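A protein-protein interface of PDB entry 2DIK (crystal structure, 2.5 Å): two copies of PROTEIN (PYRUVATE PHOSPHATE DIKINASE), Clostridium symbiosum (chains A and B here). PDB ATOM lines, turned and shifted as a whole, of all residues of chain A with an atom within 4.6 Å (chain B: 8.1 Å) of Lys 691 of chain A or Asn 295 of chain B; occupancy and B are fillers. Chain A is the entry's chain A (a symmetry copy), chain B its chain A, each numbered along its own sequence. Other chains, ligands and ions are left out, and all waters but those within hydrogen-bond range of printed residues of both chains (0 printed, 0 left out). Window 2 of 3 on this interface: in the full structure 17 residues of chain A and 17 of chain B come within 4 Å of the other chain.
Of the 14 printed residues of chain A, 5 touch a printed residue of chain B.
Printed residues of chain A that touch a printed residue of chain B: Lys 691, Glu 692, Glu 693, Thr 694 and Gly 695.
Of the 13 printed residues of chain B, 4 touch a printed residue of chain A.
Printed residues of chain B that touch a printed residue of chain A: Thr 291, Gln 292, Glu 294 and Asn 295.
Among the printed residues, no Asp or Glu carboxylate lies within 4 Å of a Lys or Arg side-chain nitrogen of the other chain.
O of Glu 693 of chain A touches OE1 of Gln 292 of chain B, 3.5 Å away.
Gln 292 of chain B touches Gly 695 of chain A (CA to CA, 3.7 Å).
Gly 695 of chain A touches Glu 294 of chain B (O to CB, 3.7 Å).
Asn 295 of chain B touches Gly 695 of chain A.
The backbone carbonyl oxygen (O) of Thr 694 of chain A is in hydrogen-bond range of the side-chain hydroxyl (OG1) of Thr 291 of chain B, 3.1 Å away.
The side-chain amide nitrogen (NE2) of Gln 292 of chain B sits at hydrogen-bond distance from the backbone carbonyl oxygen (O) of Glu 692 of chain A, 3.2 Å away.
The backbone carbonyl oxygen of Thr 694 of chain A lies within hydrogen-bond range of the backbone NH of Gln 292 of chain B, 3.3 Å away.
The side-chain amino group of Lys 691 of chain A is in hydrogen-bond range of the side-chain amide oxygen of Asn 295 of chain B, 3.3 Å away.
O of Glu 692 of chain A lies within hydrogen-bond range of ND2 of Asn 295 of chain B (2.9 Å).
The backbone carbonyl oxygen (O) of Gly 695 of chain A sits close to the backbone carbonyl oxygen (O) of Thr 291 of chain B (3.4 Å).
Of chain B, only Asn 295 comes within 4 Å of Lys 691 of chain A.
Printed residues of chain B within 4 Å of Thr 694 of chain A: Thr 291 and Gln 292.
Printed residues of chain B within 4 Å of Gly 695 of chain A: Thr 291 (3.4 Å), Gln 292 (3.7 Å), Glu 294 (3.7 Å) and Asn 295 (3.3 Å).
Of the printed residues of chain A, Thr 291 of chain B touches Thr 694 and Gly 695.
Printed residues of chain A within 4 Å of Gln 292 of chain B: Glu 692 (3.2 Å), Glu 693 (3.5 Å), Thr 694 (3.3 Å) and Gly 695 (3.7 Å).
Printed residues of chain A within 4 Å of Glu 294 of chain B: Gly 695.
Of chain A, only Lys 691 (3.3 Å), Glu 692 (2.9 Å) and Gly 695 (3.3 Å) come within 4 Å of Asn 295 of chain B.
The nearest residue of chain A that does not touch Asn 295 of chain B is Lys 731 of chain A (4.1 Å).
No position is printed for both chains.
Of the 10 pairs that touch across the chains among the printed residues, none has its exchanged pair printed and touching as well.
OE2 of Glu 693 of chain A sits close to O of Glu 689 of chain A (2.6 Å).
The backbone carbonyl oxygen of Val 690 of chain A sits close to the side-chain hydroxyl of Thr 694 of chain A (2.8 Å).
The side-chain amino group (NZ) of Lys 691 of chain A lies within salt-bridge range of the side-chain carboxylate (OD1) of Asp 697 of chain A (3.9 Å).
OG1 of Thr 694 of chain A sits at hydrogen-bond distance from N of Ile 696 of chain A (2.6 Å).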
ATOM      1  N   ALA A 687     -30.781   6.255  -1.041  1.00  0.00           N
ATOM      2  CA  ALA A 687     -29.409   6.428  -1.524  1.00  0.00           C
ATOM      3  C   ALA A 687     -28.356   6.540  -0.436  1.00  0.00           C
ATOM      4  O   ALA A 687     -27.196   6.123  -0.609  1.00  0.00           O
ATOM      5  CB  ALA A 687     -29.265   7.593  -2.494  1.00  0.00           C
ATOM      6  N   ILE A 688     -28.725   7.134   0.695  1.00  0.00           N
ATOM      7  CA  ILE A 688     -27.721   7.215   1.722  1.00  0.00           C
ATOM      8  C   ILE A 688     -27.356   5.812   2.185  1.00  0.00           C
ATOM      9  O   ILE A 688     -26.173   5.503   2.286  1.00  0.00           O
ATOM     10  CB  ILE A 688     -28.223   8.040   2.877  1.00  0.00           C
ATOM     11  CG1 ILE A 688     -28.036   9.502   2.523  1.00  0.00           C
ATOM     12  CG2 ILE A 688     -27.307   7.727   4.031  1.00  0.00           C
ATOM     13  CD1 ILE A 688     -28.830  10.466   3.388  1.00  0.00           C
ATOM     14  N   GLU A 689     -28.411   4.980   2.452  1.00  0.00           N
ATOM     15  CA  GLU A 689     -28.274   3.601   2.863  1.00  0.00           C
ATOM     16  C   GLU A 689     -27.531   2.756   1.858  1.00  0.00           C
ATOM     17  O   GLU A 689     -26.747   1.888   2.167  1.00  0.00           O
ATOM     18  CB  GLU A 689     -29.630   2.943   3.034  1.00  0.00           C
ATOM     19  CG  GLU A 689     -30.165   3.127   4.429  1.00  0.00           C
ATOM     20  CD  GLU A 689     -31.599   2.833   4.638  1.00  0.00           C
ATOM     21  OE1 GLU A 689     -32.193   1.783   4.350  1.00  0.00           O
ATOM     22  OE2 GLU A 689     -32.095   3.883   5.222  1.00  0.00           O
ATOM     23  N   VAL A 690     -27.832   2.948   0.603  1.00  0.00           N
ATOM     24  CA  VAL A 690     -27.194   2.148  -0.361  1.00  0.00           C
ATOM     25  C   VAL A 690     -25.793   2.658  -0.470  1.00  0.00           C
ATOM     26  O   VAL A 690     -24.833   1.901  -0.644  1.00  0.00           O
ATOM     27  CB  VAL A 690     -27.974   2.266  -1.625  1.00  0.00           C
ATOM     28  CG1 VAL A 690     -27.059   1.899  -2.741  1.00  0.00           C
ATOM     29  CG2 VAL A 690     -29.204   1.363  -1.548  1.00  0.00           C
ATOM     30  N   LYS A 691     -25.672   3.949  -0.274  1.00  0.00           N
ATOM     31  CA  LYS A 691     -24.353   4.497  -0.260  1.00  0.00           C
ATOM     32  C   LYS A 691     -23.656   3.869   0.917  1.00  0.00           C
ATOM     33  O   LYS A 691     -22.533   3.458   0.789  1.00  0.00           O
ATOM     34  CB  LYS A 691     -24.438   5.983  -0.088  1.00  0.00           C
ATOM     35  CG  LYS A 691     -23.329   6.781  -0.737  1.00  0.00           C
ATOM     36  CD  LYS A 691     -22.023   6.568   0.011  1.00  0.00           C
ATOM     37  CE  LYS A 691     -20.949   7.617  -0.265  1.00  0.00           C
ATOM     38  NZ  LYS A 691     -19.586   7.204   0.162  1.00  0.00           N
ATOM     39  N   GLU A 692     -24.369   3.646   2.015  1.00  0.00           N
ATOM     40  CA  GLU A 692     -23.776   3.001   3.196  1.00  0.00           C
ATOM     41  C   GLU A 692     -23.337   1.593   2.965  1.00  0.00           C
ATOM     42  O   GLU A 692     -22.190   1.273   3.223  1.00  0.00           O
ATOM     43  CB  GLU A 692     -24.694   2.875   4.421  1.00  0.00           C
ATOM     44  CG  GLU A 692     -24.674   4.103   5.350  1.00  0.00           C
ATOM     45  CD  GLU A 692     -25.914   4.229   6.205  1.00  0.00           C
ATOM     46  OE1 GLU A 692     -26.691   3.318   6.408  1.00  0.00           O
ATOM     47  OE2 GLU A 692     -26.125   5.439   6.663  1.00  0.00           O
ATOM     48  N   GLU A 693     -24.275   0.749   2.595  1.00  0.00           N
ATOM     49  CA  GLU A 693     -23.963  -0.634   2.379  1.00  0.00           C
ATOM     50  C   GLU A 693     -22.998  -0.982   1.218  1.00  0.00           C
ATOM     51  O   GLU A 693     -22.392  -2.064   1.136  1.00  0.00           O
ATOM     52  CB  GLU A 693     -25.220  -1.503   2.366  1.00  0.00           C
ATOM     53  CG  GLU A 693     -26.417  -0.839   1.694  1.00  0.00           C
ATOM     54  CD  GLU A 693     -27.748  -0.998   2.425  1.00  0.00           C
ATOM     55  OE1 GLU A 693     -28.271  -2.207   2.289  1.00  0.00           O
ATOM     56  OE2 GLU A 693     -28.367  -0.032   2.888  1.00  0.00           O
ATOM     57  N   THR A 694     -22.853  -0.099   0.250  1.00  0.00           N
ATOM     58  CA  THR A 694     -22.040  -0.472  -0.861  1.00  0.00           C
ATOM     59  C   THR A 694     -20.779   0.269  -0.829  1.00  0.00           C
ATOM     60  O   THR A 694     -19.769  -0.255  -1.231  1.00  0.00           O
ATOM     61  CB  THR A 694     -22.741  -0.058  -2.124  1.00  0.00           C
ATOM     62  OG1 THR A 694     -22.580   1.358  -2.195  1.00  0.00           O
ATOM     63  CG2 THR A 694     -24.203  -0.443  -1.976  1.00  0.00           C
ATOM     64  N   GLY A 695     -20.835   1.512  -0.436  1.00  0.00           N
ATOM     65  CA  GLY A 695     -19.634   2.268  -0.446  1.00  0.00           C
ATOM     66  C   GLY A 695     -19.493   3.052  -1.724  1.00  0.00           C
ATOM     67  O   GLY A 695     -18.529   3.904  -1.895  1.00  0.00           O
ATOM     68  N   ILE A 696     -20.512   2.824  -2.614  1.00  0.00           N
ATOM     69  CA  ILE A 696     -20.592   3.495  -3.948  1.00  0.00           C
ATOM     70  C   ILE A 696     -21.169   4.905  -3.933  1.00  0.00           C
ATOM     71  O   ILE A 696     -22.215   5.149  -3.348  1.00  0.00           O
ATOM     72  CB  ILE A 696     -21.327   2.666  -4.948  1.00  0.00           C
ATOM     73  CG1 ILE A 696     -20.514   1.409  -5.054  1.00  0.00           C
ATOM     74  CG2 ILE A 696     -21.282   3.371  -6.286  1.00  0.00           C
ATOM     75  CD1 ILE A 696     -20.404   0.944  -6.500  1.00  0.00           C
ATOM     76  N   ASP A 697     -20.511   5.844  -4.577  1.00  0.00           N
ATOM     77  CA  ASP A 697     -21.119   7.136  -4.510  1.00  0.00           C
ATOM     78  C   ASP A 697     -22.450   7.276  -5.223  1.00  0.00           C
ATOM     79  O   ASP A 697     -22.585   7.043  -6.427  1.00  0.00           O
ATOM     80  CB  ASP A 697     -20.274   8.378  -4.825  1.00  0.00           C
ATOM     81  CG  ASP A 697     -20.881   9.547  -4.054  1.00  0.00           C
ATOM     82  OD1 ASP A 697     -20.513   9.616  -2.789  1.00  0.00           O
ATOM     83  OD2 ASP A 697     -21.805  10.223  -4.468  1.00  0.00           O
ATOM     84  N   ILE A 698     -23.452   7.752  -4.483  1.00  0.00           N
ATOM     85  CA  ILE A 698     -24.683   8.072  -5.105  1.00  0.00           C
ATOM     86  C   ILE A 698     -24.867   9.578  -5.128  1.00  0.00           C
ATOM     87  O   ILE A 698     -24.464  10.218  -4.123  1.00  0.00           O
ATOM     88  CB  ILE A 698     -25.825   7.489  -4.439  1.00  0.00           C
ATOM     89  CG1 ILE A 698     -25.713   6.001  -4.535  1.00  0.00           C
ATOM     90  CG2 ILE A 698     -27.000   7.930  -5.241  1.00  0.00           C
ATOM     91  CD1 ILE A 698     -27.053   5.407  -4.139  1.00  0.00           C
ATOM     92  N   LYS A 731     -25.574  10.440   8.645  1.00  0.00           N
ATOM     93  CA  LYS A 731     -24.160  10.874   8.622  1.00  0.00           C
ATOM     94  C   LYS A 731     -23.982  12.214   7.971  1.00  0.00           C
ATOM     95  O   LYS A 731     -22.941  12.524   7.313  1.00  0.00           O
ATOM     96  CB  LYS A 731     -23.235   9.863   7.936  1.00  0.00           C
ATOM     97  CG  LYS A 731     -21.730  10.224   7.907  1.00  0.00           C
ATOM     98  CD  LYS A 731     -20.832   9.176   7.273  1.00  0.00           C
ATOM     99  CE  LYS A 731     -19.321   9.511   7.332  1.00  0.00           C
ATOM    100  NZ  LYS A 731     -18.426   8.500   6.716  1.00  0.00           N
ATOM    101  N   MET A 735     -24.387  14.111   1.202  1.00  0.00           N
ATOM    102  CA  MET A 735     -24.619  13.475  -0.046  1.00  0.00           C
ATOM    103  C   MET A 735     -24.955  14.703  -0.768  1.00  0.00           C
ATOM    104  O   MET A 735     -25.724  15.491  -0.194  1.00  0.00           O
ATOM    105  CB  MET A 735     -25.931  12.670  -0.167  1.00  0.00           C
ATOM    106  CG  MET A 735     -25.862  11.722  -1.351  1.00  0.00           C
ATOM    107  SD  MET A 735     -27.077  10.393  -1.316  1.00  0.00           S
ATOM    108  CE  MET A 735     -25.874   9.015  -1.395  1.00  0.00           C
ATOM    109  N   TYR B 271     -13.005  -7.705   1.810  1.00  0.00           N
ATOM    110  CA  TYR B 271     -12.133  -7.448   2.933  1.00  0.00           C
ATOM    111  C   TYR B 271     -12.795  -7.511   4.295  1.00  0.00           C
ATOM    112  O   TYR B 271     -14.030  -7.458   4.454  1.00  0.00           O
ATOM    113  CB  TYR B 271     -11.336  -6.163   2.826  1.00  0.00           C
ATOM    114  CG  TYR B 271     -12.186  -5.011   3.220  1.00  0.00           C
ATOM    115  CD1 TYR B 271     -13.034  -4.404   2.300  1.00  0.00           C
ATOM    116  CD2 TYR B 271     -12.070  -4.443   4.486  1.00  0.00           C
ATOM    117  CE1 TYR B 271     -13.710  -3.235   2.634  1.00  0.00           C
ATOM    118  CE2 TYR B 271     -12.779  -3.311   4.868  1.00  0.00           C
ATOM    119  CZ  TYR B 271     -13.615  -2.723   3.926  1.00  0.00           C
ATOM    120  OH  TYR B 271     -14.389  -1.668   4.280  1.00  0.00           O
ATOM    121  N   PRO B 289     -17.421  -5.455   0.747  1.00  0.00           N
ATOM    122  CA  PRO B 289     -16.996  -5.094  -0.617  1.00  0.00           C
ATOM    123  C   PRO B 289     -15.973  -3.990  -0.608  1.00  0.00           C
ATOM    124  O   PRO B 289     -16.191  -2.918  -0.054  1.00  0.00           O
ATOM    125  CB  PRO B 289     -18.249  -4.520  -1.275  1.00  0.00           C
ATOM    126  CG  PRO B 289     -19.311  -4.307  -0.194  1.00  0.00           C
ATOM    127  CD  PRO B 289     -18.838  -5.099   0.991  1.00  0.00           C
ATOM    128  N   ILE B 290     -14.888  -4.246  -1.227  1.00  0.00           N
ATOM    129  CA  ILE B 290     -13.770  -3.360  -1.241  1.00  0.00           C
ATOM    130  C   ILE B 290     -14.149  -1.899  -1.531  1.00  0.00           C
ATOM    131  O   ILE B 290     -13.461  -0.904  -1.200  1.00  0.00           O
ATOM    132  CB  ILE B 290     -12.773  -3.943  -2.209  1.00  0.00           C
ATOM    133  CG1 ILE B 290     -11.528  -3.152  -2.118  1.00  0.00           C
ATOM    134  CG2 ILE B 290     -13.316  -3.947  -3.626  1.00  0.00           C
ATOM    135  CD1 ILE B 290     -10.914  -3.385  -0.760  1.00  0.00           C
ATOM    136  N   THR B 291     -15.334  -1.744  -2.089  1.00  0.00           N
ATOM    137  CA  THR B 291     -15.816  -0.402  -2.388  1.00  0.00           C
ATOM    138  C   THR B 291     -16.280   0.328  -1.130  1.00  0.00           C
ATOM    139  O   THR B 291     -16.276   1.537  -1.012  1.00  0.00           O
ATOM    140  CB  THR B 291     -16.801  -0.441  -3.567  1.00  0.00           C
ATOM    141  OG1 THR B 291     -17.748  -1.432  -3.319  1.00  0.00           O
ATOM    142  CG2 THR B 291     -16.037  -0.992  -4.752  1.00  0.00           C
ATOM    143  N   GLN B 292     -16.636  -0.462  -0.146  1.00  0.00           N
ATOM    144  CA  GLN B 292     -17.057   0.060   1.133  1.00  0.00           C
ATOM    145  C   GLN B 292     -15.913   0.681   1.945  1.00  0.00           C
ATOM    146  O   GLN B 292     -16.121   1.552   2.761  1.00  0.00           O
ATOM    147  CB  GLN B 292     -17.666  -1.040   1.931  1.00  0.00           C
ATOM    148  CG  GLN B 292     -18.476  -0.436   3.011  1.00  0.00           C
ATOM    149  CD  GLN B 292     -19.455  -1.506   3.348  1.00  0.00           C
ATOM    150  OE1 GLN B 292     -19.383  -2.659   2.830  1.00  0.00           O
ATOM    151  NE2 GLN B 292     -20.391  -1.126   4.216  1.00  0.00           N
ATOM    152  N   LEU B 293     -14.690   0.268   1.709  1.00  0.00           N
ATOM    153  CA  LEU B 293     -13.537   0.786   2.369  1.00  0.00           C
ATOM    154  C   LEU B 293     -13.435   2.268   2.103  1.00  0.00           C
ATOM    155  O   LEU B 293     -12.610   2.981   2.647  1.00  0.00           O
ATOM    156  CB  LEU B 293     -12.338   0.019   1.771  1.00  0.00           C
ATOM    157  CG  LEU B 293     -11.000   0.063   2.502  1.00  0.00           C
ATOM    158  CD1 LEU B 293     -10.223  -1.167   2.075  1.00  0.00           C
ATOM    159  CD2 LEU B 293     -10.223   1.284   2.015  1.00  0.00           C
ATOM    160  N   GLU B 294     -14.247   2.760   1.197  1.00  0.00           N
ATOM    161  CA  GLU B 294     -14.219   4.173   0.854  1.00  0.00           C
ATOM    162  C   GLU B 294     -14.783   4.888   2.048  1.00  0.00           C
ATOM    163  O   GLU B 294     -14.357   5.972   2.471  1.00  0.00           O
ATOM    164  CB  GLU B 294     -15.198   4.369  -0.321  1.00  0.00           C
ATOM    165  CG  GLU B 294     -15.335   5.819  -0.820  1.00  0.00           C
ATOM    166  CD  GLU B 294     -14.397   6.148  -1.930  1.00  0.00           C
ATOM    167  OE1 GLU B 294     -13.171   6.466  -1.506  1.00  0.00           O
ATOM    168  OE2 GLU B 294     -14.749   6.073  -3.097  1.00  0.00           O
ATOM    169  N   ASN B 295     -15.787   4.201   2.567  1.00  0.00           N
ATOM    170  CA  ASN B 295     -16.594   4.596   3.723  1.00  0.00           C
ATOM    171  C   ASN B 295     -15.801   4.646   5.032  1.00  0.00           C
ATOM    172  O   ASN B 295     -15.684   5.717   5.621  1.00  0.00           O
ATOM    173  CB  ASN B 295     -17.825   3.662   3.909  1.00  0.00           C
ATOM    174  CG  ASN B 295     -18.851   3.771   2.783  1.00  0.00           C
ATOM    175  OD1 ASN B 295     -18.689   4.577   1.861  1.00  0.00           O
ATOM    176  ND2 ASN B 295     -19.842   2.880   2.785  1.00  0.00           N
ATOM    177  N   ASP B 296     -15.335   3.442   5.434  1.00  0.00           N
ATOM    178  CA  ASP B 296     -14.507   3.110   6.556  1.00  0.00           C
ATOM    179  C   ASP B 296     -13.215   3.902   6.624  1.00  0.00           C
ATOM    180  O   ASP B 296     -12.992   4.608   7.633  1.00  0.00           O
ATOM    181  CB  ASP B 296     -14.139   1.603   6.581  1.00  0.00           C
ATOM    182  CG  ASP B 296     -15.275   0.656   6.964  1.00  0.00           C
ATOM    183  OD1 ASP B 296     -16.453   1.283   6.997  1.00  0.00           O
ATOM    184  OD2 ASP B 296     -15.105  -0.541   7.257  1.00  0.00           O
ATOM    185  N   MET B 297     -12.375   3.769   5.590  1.00  0.00           N
ATOM    186  CA  MET B 297     -11.046   4.350   5.566  1.00  0.00           C
ATOM    187  C   MET B 297     -10.692   5.026   4.295  1.00  0.00           C
ATOM    188  O   MET B 297      -9.740   4.668   3.656  1.00  0.00           O
ATOM    189  CB  MET B 297      -9.949   3.289   5.789  1.00  0.00           C
ATOM    190  CG  MET B 297     -10.214   2.417   7.005  1.00  0.00           C
ATOM    191  SD  MET B 297      -8.836   1.399   7.603  1.00  0.00           S
ATOM    192  CE  MET B 297      -9.841  -0.072   7.976  1.00  0.00           C
ATOM    193  N   PRO B 298     -11.378   6.059   4.018  1.00  0.00           N
ATOM    194  CA  PRO B 298     -11.237   6.846   2.865  1.00  0.00           C
ATOM    195  C   PRO B 298      -9.853   7.283   2.517  1.00  0.00           C
ATOM    196  O   PRO B 298      -9.632   7.660   1.408  1.00  0.00           O
ATOM    197  CB  PRO B 298     -12.067   8.080   3.153  1.00  0.00           C
ATOM    198  CG  PRO B 298     -12.699   7.925   4.529  1.00  0.00           C
ATOM    199  CD  PRO B 298     -12.278   6.584   5.034  1.00  0.00           C
ATOM    200  N   ASP B 299      -8.896   7.354   3.392  1.00  0.00           N
ATOM    201  CA  ASP B 299      -7.596   7.846   2.929  1.00  0.00           C
ATOM    202  C   ASP B 299      -6.735   6.735   2.372  1.00  0.00           C
ATOM    203  O   ASP B 299      -5.626   6.946   1.885  1.00  0.00           O
ATOM    204  CB  ASP B 299      -6.834   8.599   4.040  1.00  0.00           C
ATOM    205  CG  ASP B 299      -7.302  10.033   4.198  1.00  0.00           C
ATOM    206  OD1 ASP B 299      -7.028  10.805   3.157  1.00  0.00           O
ATOM    207  OD2 ASP B 299      -7.956  10.419   5.167  1.00  0.00           O
ATOM    208  N   TYR B 301      -8.490   4.165   0.688  1.00  0.00           N
ATOM    209  CA  TYR B 301      -9.132   3.902  -0.531  1.00  0.00           C
ATOM    210  C   TYR B 301      -8.440   4.624  -1.644  1.00  0.00           C
ATOM    211  O   TYR B 301      -7.974   3.993  -2.568  1.00  0.00           O
ATOM    212  CB  TYR B 301     -10.580   4.326  -0.512  1.00  0.00           C
ATOM    213  CG  TYR B 301     -11.353   3.505  -1.495  1.00  0.00           C
ATOM    214  CD1 TYR B 301     -11.640   2.158  -1.270  1.00  0.00           C
ATOM    215  CD2 TYR B 301     -11.708   4.083  -2.710  1.00  0.00           C
ATOM    216  CE1 TYR B 301     -12.322   1.421  -2.237  1.00  0.00           C
ATOM    217  CE2 TYR B 301     -12.405   3.377  -3.684  1.00  0.00           C
ATOM    218  CZ  TYR B 301     -12.703   2.035  -3.436  1.00  0.00           C
ATOM    219  OH  TYR B 301     -13.472   1.354  -4.351  1.00  0.00           O
